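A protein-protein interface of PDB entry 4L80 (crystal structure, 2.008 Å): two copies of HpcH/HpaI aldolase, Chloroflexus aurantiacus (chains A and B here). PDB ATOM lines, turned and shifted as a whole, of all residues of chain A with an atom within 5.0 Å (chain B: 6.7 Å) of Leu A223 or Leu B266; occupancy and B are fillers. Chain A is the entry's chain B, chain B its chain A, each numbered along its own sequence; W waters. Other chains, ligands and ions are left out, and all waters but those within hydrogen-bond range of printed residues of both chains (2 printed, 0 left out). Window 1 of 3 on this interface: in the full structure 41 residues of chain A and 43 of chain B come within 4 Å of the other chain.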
ATOM      1  N   ARG A 189       4.379 -21.636 -28.013  1.00  0.00           N
ATOM      2  CA  ARG A 189       4.855 -22.696 -27.131  1.00  0.00           C
ATOM      3  C   ARG A 189       4.124 -22.681 -25.799  1.00  0.00           C
ATOM      4  O   ARG A 189       3.998 -23.711 -25.134  1.00  0.00           O
ATOM      5  CB  ARG A 189       6.349 -22.530 -26.866  1.00  0.00           C
ATOM      6  CG  ARG A 189       7.246 -22.851 -28.044  1.00  0.00           C
ATOM      7  CD  ARG A 189       8.649 -22.345 -27.771  1.00  0.00           C
ATOM      8  NE  ARG A 189       9.652 -22.980 -28.618  1.00  0.00           N
ATOM      9  CZ  ARG A 189      10.947 -22.680 -28.581  1.00  0.00           C
ATOM     10  NH1 ARG A 189      11.385 -21.748 -27.745  1.00  0.00           N
ATOM     11  NH2 ARG A 189      11.802 -23.305 -29.376  1.00  0.00           N
ATOM     12  N   MET A 191       5.339 -20.614 -23.514  1.00  0.00           N
ATOM     13  CA  MET A 191       6.384 -20.184 -22.592  1.00  0.00           C
ATOM     14  C   MET A 191       5.788 -19.099 -21.704  1.00  0.00           C
ATOM     15  O   MET A 191       5.294 -18.086 -22.196  1.00  0.00           O
ATOM     16  CB  MET A 191       7.603 -19.642 -23.341  1.00  0.00           C
ATOM     17  CG  MET A 191       8.286 -20.645 -24.262  1.00  0.00           C
ATOM     18  SD  MET A 191       9.717 -19.929 -25.107  1.00  0.00           S
ATOM     19  CE  MET A 191      10.918 -19.919 -23.781  1.00  0.00           C
ATOM     20  N   GLY A 198      15.790 -12.082 -24.168  1.00  0.00           N
ATOM     21  CA  GLY A 198      16.475 -11.785 -22.922  1.00  0.00           C
ATOM     22  C   GLY A 198      16.245 -12.845 -21.865  1.00  0.00           C
ATOM     23  O   GLY A 198      15.494 -13.798 -22.078  1.00  0.00           O
ATOM     24  N   GLY A 199      16.893 -12.677 -20.716  1.00  0.00           N
ATOM     25  CA  GLY A 199      16.759 -13.623 -19.626  1.00  0.00           C
ATOM     26  C   GLY A 199      15.431 -13.500 -18.899  1.00  0.00           C
ATOM     27  O   GLY A 199      14.619 -12.625 -19.203  1.00  0.00           O
ATOM     28  N   HIS A 200      15.211 -14.395 -17.944  1.00  0.00           N
ATOM     29  CA  HIS A 200      14.036 -14.351 -17.086  1.00  0.00           C
ATOM     30  C   HIS A 200      14.446 -14.880 -15.720  1.00  0.00           C
ATOM     31  O   HIS A 200      14.994 -15.978 -15.619  1.00  0.00           O
ATOM     32  CB  HIS A 200      12.898 -15.197 -17.665  1.00  0.00           C
ATOM     33  CG  HIS A 200      11.580 -14.993 -16.980  1.00  0.00           C
ATOM     34  ND1 HIS A 200      11.349 -15.375 -15.675  1.00  0.00           N
ATOM     35  CD2 HIS A 200      10.423 -14.444 -17.421  1.00  0.00           C
ATOM     36  CE1 HIS A 200      10.107 -15.070 -15.342  1.00  0.00           C
ATOM     37  NE2 HIS A 200       9.524 -14.506 -16.383  1.00  0.00           N
ATOM     38  N   TYR A 203      13.962 -18.545 -14.449  1.00  0.00           N
ATOM     39  CA  TYR A 203      14.668 -19.665 -15.069  1.00  0.00           C
ATOM     40  C   TYR A 203      16.101 -19.748 -14.574  1.00  0.00           C
ATOM     41  O   TYR A 203      16.955 -18.965 -14.990  1.00  0.00           O
ATOM     42  CB  TYR A 203      14.668 -19.545 -16.599  1.00  0.00           C
ATOM     43  CG  TYR A 203      15.233 -20.761 -17.309  1.00  0.00           C
ATOM     44  CD1 TYR A 203      15.267 -22.004 -16.685  1.00  0.00           C
ATOM     45  CD2 TYR A 203      15.740 -20.666 -18.599  1.00  0.00           C
ATOM     46  CE1 TYR A 203      15.781 -23.114 -17.325  1.00  0.00           C
ATOM     47  CE2 TYR A 203      16.254 -21.776 -19.251  1.00  0.00           C
ATOM     48  CZ  TYR A 203      16.274 -22.996 -18.609  1.00  0.00           C
ATOM     49  OH  TYR A 203      16.788 -24.103 -19.248  1.00  0.00           O
ATOM     50  N   GLN A 221      19.582 -19.156 -16.397  1.00  0.00           N
ATOM     51  CA  GLN A 221      19.873 -19.908 -17.611  1.00  0.00           C
ATOM     52  C   GLN A 221      19.281 -19.198 -18.820  1.00  0.00           C
ATOM     53  O   GLN A 221      18.367 -18.387 -18.683  1.00  0.00           O
ATOM     54  CB  GLN A 221      19.297 -21.322 -17.504  1.00  0.00           C
ATOM     55  CG  GLN A 221      19.725 -22.069 -16.252  1.00  0.00           C
ATOM     56  CD  GLN A 221      21.184 -22.480 -16.287  1.00  0.00           C
ATOM     57  OE1 GLN A 221      21.632 -23.133 -17.230  1.00  0.00           O
ATOM     58  NE2 GLN A 221      21.933 -22.100 -15.256  1.00  0.00           N
ATOM     59  N   ASP A 222      19.805 -19.510 -20.000  1.00  0.00           N
ATOM     60  CA  ASP A 222      19.333 -18.917 -21.248  1.00  0.00           C
ATOM     61  C   ASP A 222      18.110 -19.670 -21.769  1.00  0.00           C
ATOM     62  O   ASP A 222      18.170 -20.873 -22.031  1.00  0.00           O
ATOM     63  CB  ASP A 222      20.467 -18.923 -22.283  1.00  0.00           C
ATOM     64  CG  ASP A 222      20.040 -18.391 -23.645  1.00  0.00           C
ATOM     65  OD1 ASP A 222      19.035 -17.654 -23.730  1.00  0.00           O
ATOM     66  OD2 ASP A 222      20.730 -18.705 -24.638  1.00  0.00           O
ATOM     67  N   LEU A 223      17.000 -18.953 -21.909  1.00  0.00           N
ATOM     68  CA  LEU A 223      15.756 -19.534 -22.399  1.00  0.00           C
ATOM     69  C   LEU A 223      15.878 -19.996 -23.846  1.00  0.00           C
ATOM     70  O   LEU A 223      15.179 -20.914 -24.278  1.00  0.00           O
ATOM     71  CB  LEU A 223      14.625 -18.508 -22.302  1.00  0.00           C
ATOM     72  CG  LEU A 223      13.995 -18.229 -20.935  1.00  0.00           C
ATOM     73  CD1 LEU A 223      13.146 -16.973 -21.003  1.00  0.00           C
ATOM     74  CD2 LEU A 223      13.147 -19.410 -20.485  1.00  0.00           C
ATOM     75  N   TRP A 224      16.779 -19.361 -24.586  1.00  0.00           N
ATOM     76  CA  TRP A 224      16.780 -19.470 -26.039  1.00  0.00           C
ATOM     77  C   TRP A 224      17.916 -20.303 -26.615  1.00  0.00           C
ATOM     78  O   TRP A 224      18.072 -20.373 -27.835  1.00  0.00           O
ATOM     79  CB  TRP A 224      16.792 -18.068 -26.655  1.00  0.00           C
ATOM     80  CG  TRP A 224      15.640 -17.239 -26.182  1.00  0.00           C
ATOM     81  CD1 TRP A 224      15.680 -16.194 -25.302  1.00  0.00           C
ATOM     82  CD2 TRP A 224      14.265 -17.412 -26.541  1.00  0.00           C
ATOM     83  NE1 TRP A 224      14.413 -15.697 -25.104  1.00  0.00           N
ATOM     84  CE2 TRP A 224      13.528 -16.429 -25.851  1.00  0.00           C
ATOM     85  CE3 TRP A 224      13.587 -18.299 -27.384  1.00  0.00           C
ATOM     86  CZ2 TRP A 224      12.145 -16.308 -25.982  1.00  0.00           C
ATOM     87  CZ3 TRP A 224      12.215 -18.178 -27.509  1.00  0.00           C
ATOM     88  CH2 TRP A 224      11.510 -17.189 -26.813  1.00  0.00           C
ATOM     89  N   HIS A 225      18.703 -20.933 -25.748  1.00  0.00           N
ATOM     90  CA  HIS A 225      19.849 -21.714 -26.202  1.00  0.00           C
ATOM     91  C   HIS A 225      19.468 -22.760 -27.250  1.00  0.00           C
ATOM     92  O   HIS A 225      19.991 -22.754 -28.366  1.00  0.00           O
ATOM     93  CB  HIS A 225      20.540 -22.402 -25.030  1.00  0.00           C
ATOM     94  CG  HIS A 225      21.657 -23.305 -25.446  1.00  0.00           C
ATOM     95  ND1 HIS A 225      22.909 -22.835 -25.775  1.00  0.00           N
ATOM     96  CD2 HIS A 225      21.705 -24.649 -25.606  1.00  0.00           C
ATOM     97  CE1 HIS A 225      23.684 -23.852 -26.109  1.00  0.00           C
ATOM     98  NE2 HIS A 225      22.978 -24.963 -26.016  1.00  0.00           N
ATOM     99  N   THR A 227      16.694 -23.115 -28.984  1.00  0.00           N
ATOM    100  CA  THR A 227      16.024 -22.532 -30.141  1.00  0.00           C
ATOM    101  C   THR A 227      17.002 -21.908 -31.136  1.00  0.00           C
ATOM    102  O   THR A 227      16.933 -22.173 -32.337  1.00  0.00           O
ATOM    103  CB  THR A 227      14.985 -21.480 -29.709  1.00  0.00           C
ATOM    104  OG1 THR A 227      14.036 -22.084 -28.821  1.00  0.00           O
ATOM    105  CG2 THR A 227      14.254 -20.929 -30.920  1.00  0.00           C
ATOM    106  N   ASP B 222      21.857 -26.002 -16.582  1.00  0.00           N
ATOM    107  CA  ASP B 222      20.665 -26.838 -16.534  1.00  0.00           C
ATOM    108  C   ASP B 222      20.858 -28.096 -17.380  1.00  0.00           C
ATOM    109  O   ASP B 222      21.001 -28.020 -18.599  1.00  0.00           O
ATOM    110  CB  ASP B 222      19.457 -26.026 -17.014  1.00  0.00           C
ATOM    111  CG  ASP B 222      18.160 -26.820 -17.004  1.00  0.00           C
ATOM    112  OD1 ASP B 222      18.101 -27.900 -16.379  1.00  0.00           O
ATOM    113  OD2 ASP B 222      17.185 -26.342 -17.623  1.00  0.00           O
ATOM    114  N   TRP B 224      18.720 -30.212 -18.114  1.00  0.00           N
ATOM    115  CA  TRP B 224      17.481 -30.633 -18.760  1.00  0.00           C
ATOM    116  C   TRP B 224      16.929 -29.642 -19.780  1.00  0.00           C
ATOM    117  O   TRP B 224      15.821 -29.825 -20.282  1.00  0.00           O
ATOM    118  CB  TRP B 224      16.427 -30.941 -17.690  1.00  0.00           C
ATOM    119  CG  TRP B 224      16.921 -31.946 -16.701  1.00  0.00           C
ATOM    120  CD1 TRP B 224      17.318 -31.710 -15.416  1.00  0.00           C
ATOM    121  CD2 TRP B 224      17.108 -33.346 -16.930  1.00  0.00           C
ATOM    122  NE1 TRP B 224      17.730 -32.883 -14.827  1.00  0.00           N
ATOM    123  CE2 TRP B 224      17.611 -33.901 -15.737  1.00  0.00           C
ATOM    124  CE3 TRP B 224      16.894 -34.186 -18.028  1.00  0.00           C
ATOM    125  CZ2 TRP B 224      17.901 -35.257 -15.610  1.00  0.00           C
ATOM    126  CZ3 TRP B 224      17.183 -35.532 -17.899  1.00  0.00           C
ATOM    127  CH2 TRP B 224      17.681 -36.054 -16.701  1.00  0.00           C
ATOM    128  N   HIS B 225      17.703 -28.609 -20.096  1.00  0.00           N
ATOM    129  CA  HIS B 225      17.257 -27.576 -21.026  1.00  0.00           C
ATOM    130  C   HIS B 225      16.868 -28.124 -22.403  1.00  0.00           C
ATOM    131  O   HIS B 225      15.739 -27.943 -22.859  1.00  0.00           O
ATOM    132  CB  HIS B 225      18.326 -26.496 -21.182  1.00  0.00           C
ATOM    133  CG  HIS B 225      17.997 -25.479 -22.227  1.00  0.00           C
ATOM    134  ND1 HIS B 225      17.168 -24.404 -21.985  1.00  0.00           N
ATOM    135  CD2 HIS B 225      18.369 -25.382 -23.525  1.00  0.00           C
ATOM    136  CE1 HIS B 225      17.053 -23.684 -23.086  1.00  0.00           C
ATOM    137  NE2 HIS B 225      17.770 -24.257 -24.035  1.00  0.00           N
ATOM    138  N   ILE B 228      13.767 -30.665 -22.170  1.00  0.00           N
ATOM    139  CA  ILE B 228      12.476 -30.028 -21.956  1.00  0.00           C
ATOM    140  C   ILE B 228      12.062 -29.178 -23.153  1.00  0.00           C
ATOM    141  O   ILE B 228      10.908 -29.226 -23.581  1.00  0.00           O
ATOM    142  CB  ILE B 228      12.467 -29.180 -20.665  1.00  0.00           C
ATOM    143  CG1 ILE B 228      12.688 -30.079 -19.446  1.00  0.00           C
ATOM    144  CG2 ILE B 228      11.154 -28.420 -20.528  1.00  0.00           C
ATOM    145  CD1 ILE B 228      12.836 -29.321 -18.148  1.00  0.00           C
ATOM    146  N   ALA B 229      13.004 -28.414 -23.700  1.00  0.00           N
ATOM    147  CA  ALA B 229      12.727 -27.581 -24.869  1.00  0.00           C
ATOM    148  C   ALA B 229      12.238 -28.405 -26.059  1.00  0.00           C
ATOM    149  O   ALA B 229      11.281 -28.021 -26.732  1.00  0.00           O
ATOM    150  CB  ALA B 229      13.960 -26.767 -25.257  1.00  0.00           C
ATOM    151  N   VAL B 232       8.719 -29.849 -25.351  1.00  0.00           N
ATOM    152  CA  VAL B 232       7.699 -28.810 -25.476  1.00  0.00           C
ATOM    153  C   VAL B 232       7.354 -28.511 -26.937  1.00  0.00           C
ATOM    154  O   VAL B 232       6.179 -28.458 -27.300  1.00  0.00           O
ATOM    155  CB  VAL B 232       8.105 -27.513 -24.734  1.00  0.00           C
ATOM    156  CG1 VAL B 232       7.220 -26.342 -25.159  1.00  0.00           C
ATOM    157  CG2 VAL B 232       8.023 -27.722 -23.225  1.00  0.00           C
ATOM    158  N   ASP B 233       8.369 -28.335 -27.781  1.00  0.00           N
ATOM    159  CA  ASP B 233       8.114 -28.049 -29.192  1.00  0.00           C
ATOM    160  C   ASP B 233       7.333 -29.163 -29.887  1.00  0.00           C
ATOM    161  O   ASP B 233       6.372 -28.897 -30.603  1.00  0.00           O
ATOM    162  CB  ASP B 233       9.414 -27.775 -29.951  1.00  0.00           C
ATOM    163  CG  ASP B 233       9.835 -26.322 -29.877  1.00  0.00           C
ATOM    164  OD1 ASP B 233       9.078 -25.514 -29.295  1.00  0.00           O
ATOM    165  OD2 ASP B 233      10.913 -25.986 -30.412  1.00  0.00           O
ATOM    166  N   ARG B 261       9.550 -24.687 -11.580  1.00  0.00           N
ATOM    167  CA  ARG B 261       9.369 -23.381 -12.212  1.00  0.00           C
ATOM    168  C   ARG B 261      10.078 -23.268 -13.562  1.00  0.00           C
ATOM    169  O   ARG B 261       9.589 -22.602 -14.476  1.00  0.00           O
ATOM    170  CB  ARG B 261       9.751 -22.223 -11.276  1.00  0.00           C
ATOM    171  CG  ARG B 261       9.319 -20.878 -11.844  1.00  0.00           C
ATOM    172  CD  ARG B 261       9.327 -19.732 -10.831  1.00  0.00           C
ATOM    173  NE  ARG B 261       8.325 -19.905  -9.783  1.00  0.00           N
ATOM    174  CZ  ARG B 261       8.592 -20.244  -8.523  1.00  0.00           C
ATOM    175  NH1 ARG B 261       9.845 -20.459  -8.117  1.00  0.00           N
ATOM    176  NH2 ARG B 261       7.590 -20.369  -7.659  1.00  0.00           N
ATOM    177  N   ASN B 262      11.225 -23.927 -13.689  1.00  0.00           N
ATOM    178  CA  ASN B 262      11.921 -23.955 -14.968  1.00  0.00           C
ATOM    179  C   ASN B 262      11.054 -24.611 -16.035  1.00  0.00           C
ATOM    180  O   ASN B 262      10.926 -24.099 -17.147  1.00  0.00           O
ATOM    181  CB  ASN B 262      13.260 -24.682 -14.851  1.00  0.00           C
ATOM    182  CG  ASN B 262      14.256 -23.929 -14.003  1.00  0.00           C
ATOM    183  OD1 ASN B 262      14.042 -22.766 -13.658  1.00  0.00           O
ATOM    184  ND2 ASN B 262      15.360 -24.583 -13.670  1.00  0.00           N
ATOM    185  N   ALA B 263      10.454 -25.742 -15.680  1.00  0.00           N
ATOM    186  CA  ALA B 263       9.566 -26.462 -16.583  1.00  0.00           C
ATOM    187  C   ALA B 263       8.382 -25.590 -16.989  1.00  0.00           C
ATOM    188  O   ALA B 263       8.001 -25.552 -18.159  1.00  0.00           O
ATOM    189  CB  ALA B 263       9.086 -27.747 -15.936  1.00  0.00           C
ATOM    190  N   PHE B 264       7.814 -24.881 -16.016  1.00  0.00           N
ATOM    191  CA  PHE B 264       6.679 -23.996 -16.264  1.00  0.00           C
ATOM    192  C   PHE B 264       7.035 -22.869 -17.237  1.00  0.00           C
ATOM    193  O   PHE B 264       6.280 -22.579 -18.166  1.00  0.00           O
ATOM    194  CB  PHE B 264       6.157 -23.419 -14.944  1.00  0.00           C
ATOM    195  CG  PHE B 264       4.916 -22.581 -15.088  1.00  0.00           C
ATOM    196  CD1 PHE B 264       3.729 -23.144 -15.533  1.00  0.00           C
ATOM    197  CD2 PHE B 264       4.931 -21.234 -14.762  1.00  0.00           C
ATOM    198  CE1 PHE B 264       2.582 -22.375 -15.662  1.00  0.00           C
ATOM    199  CE2 PHE B 264       3.787 -20.460 -14.886  1.00  0.00           C
ATOM    200  CZ  PHE B 264       2.613 -21.033 -15.334  1.00  0.00           C
ATOM    201  N   LEU B 265       8.186 -22.240 -17.017  1.00  0.00           N
ATOM    202  CA  LEU B 265       8.658 -21.170 -17.890  1.00  0.00           C
ATOM    203  C   LEU B 265       8.835 -21.653 -19.320  1.00  0.00           C
ATOM    204  O   LEU B 265       8.536 -20.931 -20.270  1.00  0.00           O
ATOM    205  CB  LEU B 265       9.997 -20.617 -17.399  1.00  0.00           C
ATOM    206  CG  LEU B 265      10.017 -19.593 -16.272  1.00  0.00           C
ATOM    207  CD1 LEU B 265      11.216 -18.689 -16.464  1.00  0.00           C
ATOM    208  CD2 LEU B 265       8.735 -18.783 -16.240  1.00  0.00           C
ATOM    209  N   LEU B 266       9.331 -22.877 -19.463  1.00  0.00           N
ATOM    210  CA  LEU B 266       9.636 -23.433 -20.778  1.00  0.00           C
ATOM    211  C   LEU B 266       8.398 -23.923 -21.520  1.00  0.00           C
ATOM    212  O   LEU B 266       8.454 -24.183 -22.722  1.00  0.00           O
ATOM    213  CB  LEU B 266      10.678 -24.547 -20.659  1.00  0.00           C
ATOM    214  CG  LEU B 266      12.065 -24.054 -20.232  1.00  0.00           C
ATOM    215  CD1 LEU B 266      13.012 -25.217 -19.987  1.00  0.00           C
ATOM    216  CD2 LEU B 266      12.634 -23.107 -21.277  1.00  0.00           C
ATOM    217  N   GLY B 267       7.280 -24.047 -20.810  1.00  0.00           N
ATOM    218  CA  GLY B 267       6.023 -24.394 -21.451  1.00  0.00           C
ATOM    219  C   GLY B 267       5.341 -25.655 -20.951  1.00  0.00           C
ATOM    220  O   GLY B 267       4.338 -26.090 -21.519  1.00  0.00           O
ATOM    221  N   CYS B 268       5.870 -26.249 -19.890  1.00  0.00           N
ATOM    222  CA  CYS B 268       5.243 -27.441 -19.326  1.00  0.00           C
ATOM    223  C   CYS B 268       3.939 -27.096 -18.611  1.00  0.00           C
ATOM    224  O   CYS B 268       3.822 -26.045 -17.972  1.00  0.00           O
ATOM    225  CB  CYS B 268       6.200 -28.184 -18.388  1.00  0.00           C
ATOM    226  SG  CYS B 268       7.556 -29.037 -19.236  1.00  0.00           S
HETATM  227  O   HOH W   1       2.519 -24.583 -22.982  1.00  0.00           O
HETATM  228  O   HOH W   2      10.474 -25.501 -26.733  1.00  0.00           O
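OD1 of Asp B222 lies within hydrogen-bond range of N of Trp B224 (3.0 Å).
The backbone NH of His B225 sits at hydrogen-bond distance from the side-chain carboxylate of Asp B222 (3.4 Å).
The guanidinium group of Arg A189 is in hydrogen-bond range of the side-chain sulfur of Met A191.
The side-chain hydroxyl of Thr A227 sits at hydrogen-bond distance from the guanidinium group of Arg A189 (2.6 Å).
The backbone carbonyl oxygen (O) of Tyr A203 sits at hydrogen-bond distance from the backbone NH (N) of Gln A221 (3.0 Å).
OD2 of Asp A222 sits at hydrogen-bond distance from N of His A225, 3.2 Å away.
The side-chain carboxylate (OD2) of Asp B222 is in hydrogen-bond range of the side-chain hydroxyl (OH) of Tyr A203 (2.8 Å).
The side-chain amide oxygen (OE1) of Gln A221 is in hydrogen-bond range of the backbone NH (N) of Asp B222 (2.9 Å).
A ring nitrogen (ND1) of His B225 lies within hydrogen-bond range of the side-chain hydroxyl of Tyr A203 (2.8 Å).
NE of Arg A189 is in salt-bridge range of OD1 of Asp B233 (2.7 Å).
CA of Met A191 touches O of Leu B265, at 3.3 Å.
Met A191 touches Leu B266 (CG to O, 3.9 Å).
His A200 touches Leu B265 (ND1 to CD1, 3.4 Å).
Asn B262 touches Tyr A203.
Tyr A203 touches Leu B265.
O of Asp A222 touches CE1 of His B225 (3.2 Å).
O of Leu A223 touches CE1 of His B225, at 3.6 Å.
CD2 of Leu B266 touches CD2 of Leu A223, at 3.8 Å.
His A225 touches His B225 (CB to NE2, 3.5 Å).
Of chain B, only His B225 (3.6 Å) and Leu B266 (3.8 Å) come within 4 Å of Leu A223.
Printed residues of chain A within 4 Å of Leu B266: Met A191 (3.9 Å) and Leu A223 (3.8 Å).
Of the printed residues of chain A, Leu B265 touches Met A191, His A200 and Tyr A203.
Of the printed residues of chain B, Asp A222 touches His B225.
Printed residues of chain A within 4 Å of His B225: Tyr A203 (2.8 Å), Asp A222 (3.2 Å), Leu A223 (3.6 Å) and His A225 (3.5 Å).
Printed residues of chain B within 4 Å of Tyr A203: Asp B222 (2.8 Å), His B225 (2.8 Å), Asn B262 (3.4 Å) and Leu B265 (3.4 Å).
The nearest residue of chain B that does not touch Leu A223 is Leu B265 (4.5 Å).
The nearest printed residue of chain A that does not touch Leu B266 is Tyr A203 (4.01 Å).
The nearest printed residue of chain A that does not touch Asp B222 is Asp A222 (7.1 Å).
Water W2 lies within hydrogen-bond range of the backbone carbonyl oxygen of Ala B229 (2.6 Å), the side-chain carboxylate of Asp B233 (2.9 Å) and the guanidinium group of Arg A189 (3.3 Å).
Water W1 bridges the backbone carbonyl oxygen (O) of Arg A189 (2.8 Å) and the backbone carbonyl oxygen (O) of Gly B267 (2.8 Å).
Of the 15 printed residues of chain B, 6 touch a printed residue of chain A.
Hydrophobic or aromatic side chains of chain B that line the printed part of chain A: His B225, Leu B265 and Leu B266.
Hydrophobic or aromatic side chains of chain A that line the printed part of chain B: Met A191, His A200, Tyr A203, Leu A223 and His A225.
Among the printed residues, 13 pairs touch across the chains.
Among the printed residues, Asp or Glu carboxylates within 4 Å of a Lys or Arg side-chain nitrogen of the other chain: Arg A189 with Asp B233 (2.7 Å).
Asp A222 touches His B225, but with the chains exchanged His A225 does not touch Asp B222 (7.8 Å).
His B225 touches its own counterpart, His A225.
3 positions are printed for both chains.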
